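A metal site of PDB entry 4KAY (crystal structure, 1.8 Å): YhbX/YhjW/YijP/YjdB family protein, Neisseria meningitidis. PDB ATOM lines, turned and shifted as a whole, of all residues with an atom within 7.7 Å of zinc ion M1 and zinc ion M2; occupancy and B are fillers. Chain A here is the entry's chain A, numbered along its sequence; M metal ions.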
ATOM      1  N   GLY A  30      -8.572 -20.659  17.518  1.00  0.00           N
ATOM      2  CA  GLY A  30      -7.206 -20.769  18.009  1.00  0.00           C
ATOM      3  C   GLY A  30      -6.245 -19.940  17.186  1.00  0.00           C
ATOM      4  O   GLY A  30      -6.602 -19.331  16.169  1.00  0.00           O
ATOM      5  N   GLU A  31      -5.000 -19.907  17.655  1.00  0.00           N
ATOM      6  CA  GLU A  31      -3.961 -19.122  17.028  1.00  0.00           C
ATOM      7  C   GLU A  31      -2.587 -19.758  17.186  1.00  0.00           C
ATOM      8  O   GLU A  31      -2.037 -19.817  18.294  1.00  0.00           O
ATOM      9  CB  GLU A  31      -3.948 -17.708  17.610  1.00  0.00           C
ATOM     10  CG  GLU A  31      -2.794 -16.851  17.126  1.00  0.00           C
ATOM     11  CD  GLU A  31      -2.831 -16.610  15.634  1.00  0.00           C
ATOM     12  OE1 GLU A  31      -3.660 -15.778  15.185  1.00  0.00           O
ATOM     13  OE2 GLU A  31      -2.035 -17.227  14.906  1.00  0.00           O
ATOM     14  N   THR A  32      -2.037 -20.230  16.071  1.00  0.00           N
ATOM     15  CA  THR A  32      -0.642 -20.698  15.990  1.00  0.00           C
ATOM     16  C   THR A  32      -0.446 -22.099  16.569  1.00  0.00           C
ATOM     17  O   THR A  32       0.497 -22.689  16.340  1.00  0.00           O
ATOM     18  CB  THR A  32       0.339 -19.698  16.645  1.00  0.00           C
ATOM     19  OG1 THR A  32       0.205 -18.448  16.026  1.00  0.00           O
ATOM     20  CG2 THR A  32       1.771 -20.142  16.498  1.00  0.00           C
ATOM     21  N   THR A  33      -1.395 -22.589  17.305  1.00  0.00           N
ATOM     22  CA  THR A  33      -1.291 -23.908  17.896  1.00  0.00           C
ATOM     23  C   THR A  33      -1.300 -24.973  16.818  1.00  0.00           C
ATOM     24  O   THR A  33      -2.154 -24.945  15.999  1.00  0.00           O
ATOM     25  CB  THR A  33      -2.442 -24.160  18.898  1.00  0.00           C
ATOM     26  OG1 THR A  33      -2.533 -23.084  19.806  1.00  0.00           O
ATOM     27  CG2 THR A  33      -2.212 -25.377  19.663  1.00  0.00           C
ATOM     28  N   THR A  69      -1.271 -20.063   6.117  1.00  0.00           N
ATOM     29  CA  THR A  69      -0.231 -20.180   7.168  1.00  0.00           C
ATOM     30  C   THR A  69      -0.101 -18.870   7.923  1.00  0.00           C
ATOM     31  O   THR A  69       0.827 -18.656   8.741  1.00  0.00           O
ATOM     32  CB  THR A  69       1.120 -20.538   6.536  1.00  0.00           C
ATOM     33  OG1 THR A  69       1.395 -19.603   5.496  1.00  0.00           O
ATOM     34  CG2 THR A  69       1.083 -21.954   5.960  1.00  0.00           C
ATOM     35  N   SER A  70      -1.025 -17.954   7.671  1.00  0.00           N
ATOM     36  CA  SER A  70      -1.109 -16.754   8.431  1.00  0.00           C
ATOM     37  C   SER A  70      -2.552 -16.414   8.746  1.00  0.00           C
ATOM     38  O   SER A  70      -3.474 -16.832   8.046  1.00  0.00           O
ATOM     39  CB  SER A  70      -0.481 -15.590   7.676  1.00  0.00           C
ATOM     40  OG  SER A  70      -1.287 -15.292   6.546  1.00  0.00           O
ATOM     41  N   TPO A  71      -2.723 -15.601   9.774  1.00  0.00           N
ATOM     42  CA  TPO A  71      -4.020 -15.238  10.292  1.00  0.00           C
ATOM     43  CB  TPO A  71      -3.858 -14.374  11.524  1.00  0.00           C
ATOM     44  CG2 TPO A  71      -5.147 -14.342  12.345  1.00  0.00           C
ATOM     45  OG1 TPO A  71      -2.835 -14.988  12.307  1.00  0.00           O
ATOM     46  P   TPO A  71      -1.536 -13.973  12.433  1.00  0.00           P
ATOM     47  O1P TPO A  71      -1.881 -12.533  12.523  1.00  0.00           O
ATOM     48  O2P TPO A  71      -0.940 -14.475  13.828  1.00  0.00           O
ATOM     49  O3P TPO A  71      -0.445 -14.213  11.258  1.00  0.00           O
ATOM     50  C   TPO A  71      -4.839 -14.510   9.240  1.00  0.00           C
ATOM     51  O   TPO A  71      -5.998 -14.772   9.099  1.00  0.00           O
ATOM     52  N   ALA A  72      -4.226 -13.549   8.559  1.00  0.00           N
ATOM     53  CA  ALA A  72      -4.979 -12.693   7.664  1.00  0.00           C
ATOM     54  C   ALA A  72      -5.474 -13.499   6.480  1.00  0.00           C
ATOM     55  O   ALA A  72      -6.401 -13.044   5.780  1.00  0.00           O
ATOM     56  CB  ALA A  72      -4.132 -11.503   7.205  1.00  0.00           C
ATOM     57  N   HIS A  73      -4.849 -14.643   6.199  1.00  0.00           N
ATOM     58  CA  HIS A  73      -5.323 -15.551   5.156  1.00  0.00           C
ATOM     59  C   HIS A  73      -6.357 -16.533   5.726  1.00  0.00           C
ATOM     60  O   HIS A  73      -7.486 -16.629   5.222  1.00  0.00           O
ATOM     61  CB  HIS A  73      -4.159 -16.329   4.536  1.00  0.00           C
ATOM     62  CG  HIS A  73      -4.547 -17.138   3.326  1.00  0.00           C
ATOM     63  ND1 HIS A  73      -4.295 -16.716   2.043  1.00  0.00           N
ATOM     64  CD2 HIS A  73      -5.215 -18.309   3.216  1.00  0.00           C
ATOM     65  CE1 HIS A  73      -4.750 -17.609   1.189  1.00  0.00           C
ATOM     66  NE2 HIS A  73      -5.308 -18.586   1.867  1.00  0.00           N
ATOM     67  N   SER A  74      -5.978 -17.277   6.757  1.00  0.00           N
ATOM     68  CA  SER A  74      -6.874 -18.308   7.282  1.00  0.00           C
ATOM     69  C   SER A  74      -8.225 -17.829   7.787  1.00  0.00           C
ATOM     70  O   SER A  74      -9.255 -18.511   7.560  1.00  0.00           O
ATOM     71  CB  SER A  74      -6.173 -19.103   8.376  1.00  0.00           C
ATOM     72  OG  SER A  74      -5.126 -19.880   7.841  1.00  0.00           O
ATOM     73  N   LEU A  75      -8.284 -16.711   8.502  1.00  0.00           N
ATOM     74  CA  LEU A  75      -9.534 -16.322   9.125  1.00  0.00           C
ATOM     75  C   LEU A  75     -10.555 -15.960   8.049  1.00  0.00           C
ATOM     76  O   LEU A  75     -11.678 -16.447   8.043  1.00  0.00           O
ATOM     77  CB  LEU A  75      -9.389 -15.151  10.076  1.00  0.00           C
ATOM     78  CG  LEU A  75      -9.719 -15.510  11.521  1.00  0.00           C
ATOM     79  CD1 LEU A  75      -8.651 -16.463  12.025  1.00  0.00           C
ATOM     80  CD2 LEU A  75      -9.760 -14.226  12.357  1.00  0.00           C
ATOM     81  N   ASP A 115      -6.987 -11.190  19.844  1.00  0.00           N
ATOM     82  CA  ASP A 115      -5.848 -11.590  18.993  1.00  0.00           C
ATOM     83  C   ASP A 115      -5.417 -10.505  17.958  1.00  0.00           C
ATOM     84  O   ASP A 115      -4.913 -10.803  16.854  1.00  0.00           O
ATOM     85  CB  ASP A 115      -6.191 -12.909  18.294  1.00  0.00           C
ATOM     86  CG  ASP A 115      -5.031 -13.542  17.553  1.00  0.00           C
ATOM     87  OD1 ASP A 115      -3.861 -13.467  18.016  1.00  0.00           O
ATOM     88  OD2 ASP A 115      -5.289 -14.156  16.477  1.00  0.00           O
ATOM     89  N   SER A 116      -5.596  -9.257  18.345  1.00  0.00           N
ATOM     90  CA  SER A 116      -5.132  -8.080  17.566  1.00  0.00           C
ATOM     91  C   SER A 116      -6.032  -7.690  16.377  1.00  0.00           C
ATOM     92  O   SER A 116      -5.810  -6.635  15.768  1.00  0.00           O
ATOM     93  CB  SER A 116      -3.686  -8.230  17.048  1.00  0.00           C
ATOM     94  OG  SER A 116      -3.623  -8.807  15.752  1.00  0.00           O
ATOM     95  N   LYS A 119      -9.836  -9.380  11.341  1.00  0.00           N
ATOM     96  CA  LYS A 119      -9.462  -9.491   9.933  1.00  0.00           C
ATOM     97  C   LYS A 119     -10.659  -9.301   9.000  1.00  0.00           C
ATOM     98  O   LYS A 119     -10.831 -10.046   8.007  1.00  0.00           O
ATOM     99  CB  LYS A 119      -8.827 -10.850   9.642  1.00  0.00           C
ATOM    100  CG  LYS A 119      -7.648 -11.193  10.531  1.00  0.00           C
ATOM    101  CD  LYS A 119      -6.578 -10.107  10.484  1.00  0.00           C
ATOM    102  CE  LYS A 119      -5.229 -10.620  11.014  1.00  0.00           C
ATOM    103  NZ  LYS A 119      -4.214  -9.541  11.082  1.00  0.00           N
ATOM    104  N   HIS A 169     -12.058 -15.370  19.899  1.00  0.00           N
ATOM    105  CA  HIS A 169     -10.868 -15.392  19.069  1.00  0.00           C
ATOM    106  C   HIS A 169      -9.651 -15.185  19.940  1.00  0.00           C
ATOM    107  O   HIS A 169      -9.419 -14.080  20.456  1.00  0.00           O
ATOM    108  CB  HIS A 169     -10.922 -14.281  17.994  1.00  0.00           C
ATOM    109  CG  HIS A 169      -9.764 -14.340  17.035  1.00  0.00           C
ATOM    110  ND1 HIS A 169      -9.356 -13.249  16.288  1.00  0.00           N
ATOM    111  CD2 HIS A 169      -8.930 -15.358  16.702  1.00  0.00           C
ATOM    112  CE1 HIS A 169      -8.329 -13.597  15.543  1.00  0.00           C
ATOM    113  NE2 HIS A 169      -8.063 -14.878  15.761  1.00  0.00           N
ATOM    114  N   THR A 170      -8.907 -16.259  20.140  1.00  0.00           N
ATOM    115  CA  THR A 170      -7.791 -16.261  21.064  1.00  0.00           C
ATOM    116  C   THR A 170      -6.437 -15.913  20.465  1.00  0.00           C
ATOM    117  O   THR A 170      -6.246 -15.968  19.235  1.00  0.00           O
ATOM    118  CB  THR A 170      -7.687 -17.675  21.657  1.00  0.00           C
ATOM    119  OG1 THR A 170      -7.376 -18.599  20.595  1.00  0.00           O
ATOM    120  CG2 THR A 170      -8.990 -18.046  22.319  1.00  0.00           C
ATOM    121  N   ILE A 171      -5.477 -15.573  21.356  1.00  0.00           N
ATOM    122  CA  ILE A 171      -4.086 -15.370  20.974  1.00  0.00           C
ATOM    123  C   ILE A 171      -3.263 -16.644  21.075  1.00  0.00           C
ATOM    124  O   ILE A 171      -2.220 -16.802  20.408  1.00  0.00           O
ATOM    125  CB  ILE A 171      -3.448 -14.159  21.735  1.00  0.00           C
ATOM    126  CG1 ILE A 171      -2.100 -13.833  21.106  1.00  0.00           C
ATOM    127  CG2 ILE A 171      -3.322 -14.413  23.227  1.00  0.00           C
ATOM    128  CD1 ILE A 171      -1.622 -12.413  21.465  1.00  0.00           C
ATOM    129  N   HIS A 174       0.639 -17.717  19.982  1.00  0.00           N
ATOM    130  CA  HIS A 174       1.333 -16.751  19.144  1.00  0.00           C
ATOM    131  C   HIS A 174       2.674 -16.369  19.761  1.00  0.00           C
ATOM    132  O   HIS A 174       2.772 -16.130  20.959  1.00  0.00           O
ATOM    133  CB  HIS A 174       0.500 -15.517  18.921  1.00  0.00           C
ATOM    134  CG  HIS A 174       0.790 -14.830  17.627  1.00  0.00           C
ATOM    135  ND1 HIS A 174       1.930 -14.073  17.416  1.00  0.00           N
ATOM    136  CD2 HIS A 174       0.100 -14.780  16.452  1.00  0.00           C
ATOM    137  CE1 HIS A 174       1.927 -13.599  16.182  1.00  0.00           C
ATOM    138  NE2 HIS A 174       0.829 -14.020  15.571  1.00  0.00           N
ATOM    139  N   GLY A 175       3.688 -16.326  18.913  1.00  0.00           N
ATOM    140  CA  GLY A 175       5.028 -15.881  19.290  1.00  0.00           C
ATOM    141  C   GLY A 175       5.377 -14.548  18.625  1.00  0.00           C
ATOM    142  O   GLY A 175       4.547 -13.934  17.930  1.00  0.00           O
ATOM    143  N   SER A 242      -7.489 -24.314  15.373  1.00  0.00           N
ATOM    144  CA  SER A 242      -6.470 -23.272  15.209  1.00  0.00           C
ATOM    145  C   SER A 242      -6.520 -22.650  13.803  1.00  0.00           C
ATOM    146  O   SER A 242      -7.103 -23.229  12.879  1.00  0.00           O
ATOM    147  CB  SER A 242      -5.068 -23.837  15.432  1.00  0.00           C
ATOM    148  OG  SER A 242      -4.149 -22.769  15.552  1.00  0.00           O
ATOM    149  N   ASP A 243      -5.941 -21.458  13.658  1.00  0.00           N
ATOM    150  CA  ASP A 243      -5.850 -20.839  12.322  1.00  0.00           C
ATOM    151  C   ASP A 243      -4.718 -21.340  11.428  1.00  0.00           C
ATOM    152  O   ASP A 243      -4.807 -21.256  10.197  1.00  0.00           O
ATOM    153  CB  ASP A 243      -5.827 -19.306  12.423  1.00  0.00           C
ATOM    154  CG  ASP A 243      -4.575 -18.774  13.057  1.00  0.00           C
ATOM    155  OD1 ASP A 243      -3.901 -19.497  13.847  1.00  0.00           O
ATOM    156  OD2 ASP A 243      -4.329 -17.580  12.834  1.00  0.00           O
ATOM    157  N   HIS A 244      -3.670 -21.869  12.044  1.00  0.00           N
ATOM    158  CA  HIS A 244      -2.484 -22.373  11.372  1.00  0.00           C
ATOM    159  C   HIS A 244      -1.557 -22.788  12.480  1.00  0.00           C
ATOM    160  O   HIS A 244      -1.801 -22.461  13.646  1.00  0.00           O
ATOM    161  CB  HIS A 244      -1.783 -21.282  10.533  1.00  0.00           C
ATOM    162  CG  HIS A 244      -1.469 -20.006  11.307  1.00  0.00           C
ATOM    163  ND1 HIS A 244      -0.411 -19.897  12.202  1.00  0.00           N
ATOM    164  CD2 HIS A 244      -2.079 -18.803  11.296  1.00  0.00           C
ATOM    165  CE1 HIS A 244      -0.420 -18.690  12.731  1.00  0.00           C
ATOM    166  NE2 HIS A 244      -1.424 -17.999  12.206  1.00  0.00           N
ATOM    167  N   GLY A 245      -0.477 -23.454  12.103  1.00  0.00           N
ATOM    168  CA  GLY A 245       0.548 -23.887  13.019  1.00  0.00           C
ATOM    169  C   GLY A 245       1.741 -22.949  13.119  1.00  0.00           C
ATOM    170  O   GLY A 245       1.628 -21.747  12.928  1.00  0.00           O
ATOM    171  N   GLU A 246       2.885 -23.555  13.431  1.00  0.00           N
ATOM    172  CA  GLU A 246       4.075 -22.793  13.730  1.00  0.00           C
ATOM    173  C   GLU A 246       5.264 -23.680  13.419  1.00  0.00           C
ATOM    174  O   GLU A 246       5.205 -24.909  13.544  1.00  0.00           O
ATOM    175  CB  GLU A 246       4.094 -22.493  15.252  1.00  0.00           C
ATOM    176  CG  GLU A 246       5.193 -21.469  15.697  1.00  0.00           C
ATOM    177  CD  GLU A 246       4.873 -20.038  15.314  1.00  0.00           C
ATOM    178  OE1 GLU A 246       4.185 -19.815  14.299  1.00  0.00           O
ATOM    179  OE2 GLU A 246       5.309 -19.089  16.021  1.00  0.00           O
ATOM    180  N   LEU A 255       8.535 -19.277  13.345  1.00  0.00           N
ATOM    181  CA  LEU A 255       7.284 -18.523  13.197  1.00  0.00           C
ATOM    182  C   LEU A 255       6.421 -19.204  12.138  1.00  0.00           C
ATOM    183  O   LEU A 255       6.459 -20.380  12.031  1.00  0.00           O
ATOM    184  CB  LEU A 255       7.607 -17.053  12.901  1.00  0.00           C
ATOM    185  CG  LEU A 255       8.576 -16.335  13.805  1.00  0.00           C
ATOM    186  CD1 LEU A 255       8.809 -14.899  13.356  1.00  0.00           C
ATOM    187  CD2 LEU A 255       8.054 -16.339  15.197  1.00  0.00           C
ATOM    188  N   HIS A 256       5.576 -18.434  11.457  1.00  0.00           N
ATOM    189  CA  HIS A 256       4.699 -18.998  10.461  1.00  0.00           C
ATOM    190  C   HIS A 256       4.721 -18.202   9.129  1.00  0.00           C
ATOM    191  O   HIS A 256       5.733 -17.682   8.764  1.00  0.00           O
ATOM    192  CB  HIS A 256       3.316 -19.195  11.117  1.00  0.00           C
ATOM    193  CG  HIS A 256       2.772 -17.984  11.767  1.00  0.00           C
ATOM    194  ND1 HIS A 256       2.936 -17.753  13.105  1.00  0.00           N
ATOM    195  CD2 HIS A 256       2.018 -16.955  11.311  1.00  0.00           C
ATOM    196  CE1 HIS A 256       2.324 -16.640  13.429  1.00  0.00           C
ATOM    197  NE2 HIS A 256       1.773 -16.132  12.354  1.00  0.00           N
ATOM    198  N   ALA A 257       3.600 -18.162   8.435  1.00  0.00           N
ATOM    199  CA  ALA A 257       3.492 -17.431   7.161  1.00  0.00           C
ATOM    200  C   ALA A 257       4.421 -17.952   6.039  1.00  0.00           C
ATOM    201  O   ALA A 257       4.662 -17.262   5.090  1.00  0.00           O
ATOM    202  CB  ALA A 257       3.757 -15.966   7.406  1.00  0.00           C
HETATM  203 ZN    ZN M   1       0.938 -14.204  13.366  1.00  0.00          ZN
HETATM  204 ZN    ZN M   2      -2.585 -16.731  13.216  1.00  0.00          ZN
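The backbone NH (N) of Asp 243 lies within hydrogen-bond range of the backbone carbonyl oxygen (O) of Gly 30 (3.4 Å). The backbone carbonyl oxygen (O) of Asp 243 lies within hydrogen-bond range of the side-chain hydroxyl (OG) of Ser 74 (2.7 Å). O of His 244 is in hydrogen-bond range of OG of Ser 242, at 3.0 Å. The side-chain hydroxyl of Thr 32 sits close to the side-chain carboxylate of Glu 31 (2.8 Å). The backbone carbonyl oxygen of His 244 sits close to the backbone NH of Thr 32 (3.3 Å). OE1 of Glu 31 lies close to OD2 of Asp 115. The side-chain carboxylate (OD1) of Asp 243 is in hydrogen-bond range of the backbone NH (N) of Thr 32 (3.0 Å). A ring nitrogen (ND1) of His 256 sits at hydrogen-bond distance from the side-chain carboxylate of Glu 246.
Zinc ion M2 is bound by the side-chain carboxylate (OE2) of Glu 31, 1.8 Å away. Zinc ion M2 is bound by the side-chain carboxylate (OD2) of Asp 243, 2.0 Å away. Zinc ion M2 is bound by OG1 of TPO 71, 2.0 Å away. Zinc ion M2 is bound by a ring nitrogen (NE2) of His 244, at 2.0 Å. Zinc ion M2 is bound by the side-chain carboxylate (OE1) of Glu 31, 2.4 Å away.
Three residues have an atom within 4 Å of zinc ion M1: TPO 71, His 174 and His 256. The nearest printed residue that does not touch zinc ion M1 is Glu 31 (4.5 Å).
Within 4 Å of zinc ion M2: Glu 31, TPO 71, Asp 243 and His 244. Along chain A the residues within 4 Å of zinc ion M2 span positions 31 to 244.
O2P of TPO 71 is bound to zinc ion M1, 2.0 Å away. NE2 of His 174 binds zinc ion M1 (2.2 Å). Zinc ion M1 is bound by NE2 of His 256. O3P of TPO 71 binds zinc ion M1, at 2.5 Å.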
